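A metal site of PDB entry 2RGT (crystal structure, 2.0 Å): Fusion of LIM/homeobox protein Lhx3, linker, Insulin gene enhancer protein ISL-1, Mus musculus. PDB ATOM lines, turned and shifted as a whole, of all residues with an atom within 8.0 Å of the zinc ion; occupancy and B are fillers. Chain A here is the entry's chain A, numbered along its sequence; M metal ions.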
ATOM      1  N   LYS A  35     -23.633 -22.090  -7.927  1.00  0.00           N
ATOM      2  CA  LYS A  35     -24.536 -21.339  -8.771  1.00  0.00           C
ATOM      3  C   LYS A  35     -25.901 -21.268  -8.060  1.00  0.00           C
ATOM      4  O   LYS A  35     -26.187 -22.056  -7.124  1.00  0.00           O
ATOM      5  CB  LYS A  35     -24.673 -22.023 -10.128  1.00  0.00           C
ATOM      6  CG  LYS A  35     -25.454 -23.321 -10.037  1.00  0.00           C
ATOM      7  CD  LYS A  35     -25.373 -24.111 -11.314  1.00  0.00           C
ATOM      8  CE  LYS A  35     -25.620 -25.563 -11.016  1.00  0.00           C
ATOM      9  NZ  LYS A  35     -25.456 -26.387 -12.246  1.00  0.00           N
ATOM     10  N   CYS A  36     -26.729 -20.306  -8.500  1.00  0.00           N
ATOM     11  CA  CYS A  36     -28.053 -20.122  -7.956  1.00  0.00           C
ATOM     12  C   CYS A  36     -28.899 -21.390  -8.131  1.00  0.00           C
ATOM     13  O   CYS A  36     -29.009 -21.943  -9.232  1.00  0.00           O
ATOM     14  CB  CYS A  36     -28.738 -18.930  -8.595  1.00  0.00           C
ATOM     15  SG  CYS A  36     -30.395 -18.580  -7.906  1.00  0.00           S
ATOM     16  N   SER A  37     -29.460 -21.876  -7.033  1.00  0.00           N
ATOM     17  CA  SER A  37     -30.363 -23.034  -7.061  1.00  0.00           C
ATOM     18  C   SER A  37     -31.465 -22.853  -8.125  1.00  0.00           C
ATOM     19  O   SER A  37     -31.796 -23.814  -8.820  1.00  0.00           O
ATOM     20  CB  SER A  37     -30.962 -23.270  -5.662  1.00  0.00           C
ATOM     21  OG  SER A  37     -31.812 -24.408  -5.629  1.00  0.00           O
ATOM     22  N   ASP A  38     -31.979 -21.628  -8.290  1.00  0.00           N
ATOM     23  CA  ASP A  38     -33.111 -21.342  -9.174  1.00  0.00           C
ATOM     24  C   ASP A  38     -32.767 -20.858 -10.594  1.00  0.00           C
ATOM     25  O   ASP A  38     -33.450 -21.253 -11.525  1.00  0.00           O
ATOM     26  CB  ASP A  38     -34.093 -20.354  -8.534  1.00  0.00           C
ATOM     27  CG  ASP A  38     -34.789 -20.903  -7.293  1.00  0.00           C
ATOM     28  OD1 ASP A  38     -34.816 -22.150  -7.105  1.00  0.00           O
ATOM     29  OD2 ASP A  38     -35.299 -20.086  -6.480  1.00  0.00           O
ATOM     30  N   CYS A  39     -31.760 -19.996 -10.778  1.00  0.00           N
ATOM     31  CA  CYS A  39     -31.414 -19.570 -12.152  1.00  0.00           C
ATOM     32  C   CYS A  39     -30.128 -20.176 -12.678  1.00  0.00           C
ATOM     33  O   CYS A  39     -29.729 -19.916 -13.802  1.00  0.00           O
ATOM     34  CB  CYS A  39     -31.406 -18.037 -12.293  1.00  0.00           C
ATOM     35  SG  CYS A  39     -30.147 -17.097 -11.350  1.00  0.00           S
ATOM     36  N   HIS A  40     -29.469 -20.979 -11.849  1.00  0.00           N
ATOM     37  CA  HIS A  40     -28.200 -21.592 -12.222  1.00  0.00           C
ATOM     38  C   HIS A  40     -27.223 -20.569 -12.768  1.00  0.00           C
ATOM     39  O   HIS A  40     -26.520 -20.816 -13.747  1.00  0.00           O
ATOM     40  CB  HIS A  40     -28.438 -22.699 -13.258  1.00  0.00           C
ATOM     41  CG  HIS A  40     -29.163 -23.894 -12.725  1.00  0.00           C
ATOM     42  ND1 HIS A  40     -29.244 -25.090 -13.403  1.00  0.00           N
ATOM     43  CD2 HIS A  40     -29.846 -24.075 -11.564  1.00  0.00           C
ATOM     44  CE1 HIS A  40     -29.944 -25.949 -12.695  1.00  0.00           C
ATOM     45  NE2 HIS A  40     -30.323 -25.359 -11.568  1.00  0.00           N
ATOM     46  N   VAL A  41     -27.186 -19.400 -12.131  1.00  0.00           N
ATOM     47  CA  VAL A  41     -26.126 -18.423 -12.372  1.00  0.00           C
ATOM     48  C   VAL A  41     -25.044 -18.510 -11.305  1.00  0.00           C
ATOM     49  O   VAL A  41     -25.335 -18.650 -10.114  1.00  0.00           O
ATOM     50  CB  VAL A  41     -26.678 -16.987 -12.419  1.00  0.00           C
ATOM     51  CG1 VAL A  41     -27.308 -16.621 -11.085  1.00  0.00           C
ATOM     52  CG2 VAL A  41     -25.573 -16.008 -12.781  1.00  0.00           C
ATOM     53  N   PRO A  42     -23.791 -18.434 -11.734  1.00  0.00           N
ATOM     54  CA  PRO A  42     -22.652 -18.668 -10.839  1.00  0.00           C
ATOM     55  C   PRO A  42     -22.548 -17.588  -9.769  1.00  0.00           C
ATOM     56  O   PRO A  42     -22.698 -16.406 -10.069  1.00  0.00           O
ATOM     57  CB  PRO A  42     -21.445 -18.601 -11.778  1.00  0.00           C
ATOM     58  CG  PRO A  42     -21.888 -17.707 -12.877  1.00  0.00           C
ATOM     59  CD  PRO A  42     -23.356 -17.979 -13.066  1.00  0.00           C
ATOM     60  N   LEU A  43     -22.278 -17.990  -8.529  1.00  0.00           N
ATOM     61  CA  LEU A  43     -22.267 -17.063  -7.404  1.00  0.00           C
ATOM     62  C   LEU A  43     -20.846 -16.596  -7.082  1.00  0.00           C
ATOM     63  O   LEU A  43     -19.934 -17.435  -6.983  1.00  0.00           O
ATOM     64  CB  LEU A  43     -22.919 -17.718  -6.187  1.00  0.00           C
ATOM     65  CG  LEU A  43     -24.390 -18.042  -6.483  1.00  0.00           C
ATOM     66  CD1 LEU A  43     -25.060 -18.840  -5.374  1.00  0.00           C
ATOM     67  CD2 LEU A  43     -25.129 -16.780  -6.714  1.00  0.00           C
ATOM     68  N   VAL A  54     -28.429 -22.513  -2.071  1.00  0.00           N
ATOM     69  CA  VAL A  54     -27.873 -21.185  -2.256  1.00  0.00           C
ATOM     70  C   VAL A  54     -28.586 -20.516  -3.402  1.00  0.00           C
ATOM     71  O   VAL A  54     -28.992 -21.166  -4.380  1.00  0.00           O
ATOM     72  CB  VAL A  54     -26.335 -21.184  -2.527  1.00  0.00           C
ATOM     73  CG1 VAL A  54     -25.579 -21.682  -1.329  1.00  0.00           C
ATOM     74  CG2 VAL A  54     -25.986 -22.061  -3.725  1.00  0.00           C
ATOM     75  N   TYR A  55     -28.704 -19.190  -3.281  1.00  0.00           N
ATOM     76  CA  TYR A  55     -29.450 -18.336  -4.206  1.00  0.00           C
ATOM     77  C   TYR A  55     -28.636 -17.090  -4.489  1.00  0.00           C
ATOM     78  O   TYR A  55     -27.898 -16.604  -3.619  1.00  0.00           O
ATOM     79  CB  TYR A  55     -30.809 -17.934  -3.610  1.00  0.00           C
ATOM     80  CG  TYR A  55     -31.664 -19.130  -3.219  1.00  0.00           C
ATOM     81  CD1 TYR A  55     -32.459 -19.790  -4.169  1.00  0.00           C
ATOM     82  CD2 TYR A  55     -31.628 -19.641  -1.901  1.00  0.00           C
ATOM     83  CE1 TYR A  55     -33.231 -20.940  -3.786  1.00  0.00           C
ATOM     84  CE2 TYR A  55     -32.387 -20.764  -1.525  1.00  0.00           C
ATOM     85  CZ  TYR A  55     -33.191 -21.410  -2.465  1.00  0.00           C
ATOM     86  OH  TYR A  55     -33.934 -22.501  -2.079  1.00  0.00           O
ATOM     87  N   CYS A  56     -28.715 -16.636  -5.724  1.00  0.00           N
ATOM     88  CA  CYS A  56     -28.443 -15.250  -6.043  1.00  0.00           C
ATOM     89  C   CYS A  56     -29.498 -14.334  -5.389  1.00  0.00           C
ATOM     90  O   CYS A  56     -30.605 -14.760  -5.114  1.00  0.00           O
ATOM     91  CB  CYS A  56     -28.483 -15.063  -7.554  1.00  0.00           C
ATOM     92  SG  CYS A  56     -30.165 -14.757  -8.206  1.00  0.00           S
ATOM     93  N   LYS A  57     -29.144 -13.076  -5.183  1.00  0.00           N
ATOM     94  CA  LYS A  57     -30.023 -12.084  -4.554  1.00  0.00           C
ATOM     95  C   LYS A  57     -31.449 -11.940  -5.128  1.00  0.00           C
ATOM     96  O   LYS A  57     -32.413 -11.923  -4.381  1.00  0.00           O
ATOM     97  CB  LYS A  57     -29.293 -10.722  -4.565  1.00  0.00           C
ATOM     98  CG  LYS A  57     -29.814  -9.675  -3.597  1.00  0.00           C
ATOM     99  CD  LYS A  57     -28.998  -8.369  -3.745  1.00  0.00           C
ATOM    100  CE  LYS A  57     -29.076  -7.534  -2.473  1.00  0.00           C
ATOM    101  NZ  LYS A  57     -27.855  -6.737  -2.178  1.00  0.00           N
ATOM    102  N   ASP A  58     -31.591 -11.730  -6.428  1.00  0.00           N
ATOM    103  CA  ASP A  58     -32.907 -11.656  -7.077  1.00  0.00           C
ATOM    104  C   ASP A  58     -33.777 -12.819  -6.567  1.00  0.00           C
ATOM    105  O   ASP A  58     -34.815 -12.625  -5.928  1.00  0.00           O
ATOM    106  CB  ASP A  58     -32.813 -11.709  -8.632  1.00  0.00           C
ATOM    107  CG  ASP A  58     -32.140 -10.443  -9.259  1.00  0.00           C
ATOM    108  OD1 ASP A  58     -32.185  -9.346  -8.656  1.00  0.00           O
ATOM    109  OD2 ASP A  58     -31.554 -10.540 -10.387  1.00  0.00           O
ATOM    110  N   ASP A  59     -33.318 -14.047  -6.849  1.00  0.00           N
ATOM    111  CA  ASP A  59     -34.125 -15.226  -6.617  1.00  0.00           C
ATOM    112  C   ASP A  59     -34.406 -15.466  -5.132  1.00  0.00           C
ATOM    113  O   ASP A  59     -35.450 -16.040  -4.802  1.00  0.00           O
ATOM    114  CB  ASP A  59     -33.515 -16.466  -7.259  1.00  0.00           C
ATOM    115  CG  ASP A  59     -33.752 -16.513  -8.777  1.00  0.00           C
ATOM    116  OD1 ASP A  59     -32.775 -16.752  -9.529  1.00  0.00           O
ATOM    117  OD2 ASP A  59     -34.919 -16.345  -9.222  1.00  0.00           O
ATOM    118  N   PHE A  60     -33.502 -15.013  -4.277  1.00  0.00           N
ATOM    119  CA  PHE A  60     -33.702 -15.142  -2.817  1.00  0.00           C
ATOM    120  C   PHE A  60     -34.912 -14.297  -2.386  1.00  0.00           C
ATOM    121  O   PHE A  60     -35.659 -14.710  -1.510  1.00  0.00           O
ATOM    122  CB  PHE A  60     -32.457 -14.724  -2.029  1.00  0.00           C
ATOM    123  CG  PHE A  60     -32.594 -14.866  -0.531  1.00  0.00           C
ATOM    124  CD1 PHE A  60     -32.346 -16.088   0.100  1.00  0.00           C
ATOM    125  CD2 PHE A  60     -32.975 -13.766   0.252  1.00  0.00           C
ATOM    126  CE1 PHE A  60     -32.497 -16.245   1.467  1.00  0.00           C
ATOM    127  CE2 PHE A  60     -33.117 -13.889   1.618  1.00  0.00           C
ATOM    128  CZ  PHE A  60     -32.873 -15.153   2.245  1.00  0.00           C
ATOM    129  N   LYS A  62     -37.379 -13.111  -4.437  1.00  0.00           N
ATOM    130  CA  LYS A  62     -38.521 -13.650  -5.152  1.00  0.00           C
ATOM    131  C   LYS A  62     -39.098 -14.826  -4.406  1.00  0.00           C
ATOM    132  O   LYS A  62     -40.294 -15.044  -4.398  1.00  0.00           O
ATOM    133  CB  LYS A  62     -38.080 -14.118  -6.536  1.00  0.00           C
ATOM    134  CG  LYS A  62     -38.121 -13.072  -7.617  1.00  0.00           C
ATOM    135  CD  LYS A  62     -36.948 -13.206  -8.557  1.00  0.00           C
ATOM    136  CE  LYS A  62     -37.356 -13.819  -9.871  1.00  0.00           C
ATOM    137  NZ  LYS A  62     -36.997 -12.958 -11.026  1.00  0.00           N
HETATM  138 ZN    ZN M   1     -30.686 -16.816  -9.185  1.00  0.00          ZN
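The backbone NH of Cys 36 lies within hydrogen-bond range of the backbone carbonyl oxygen of Val 41.
SG of Cys 36 lies close to N of Asp 38, at 3.5 Å.
The side-chain sulfur of Cys 56 sits close to the backbone NH of Asp 58, at 3.8 Å.
Val 41 touches the zinc ion.
Of the 17 residues printed, 5 come within 4 Å of the zinc ion.
The zinc ion is bound by OD1 of Asp 59 (2.1 Å), SG of Cys 36 (2.2 Å), SG of Cys 39 (2.2 Å) and SG of Cys 56 (2.3 Å).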
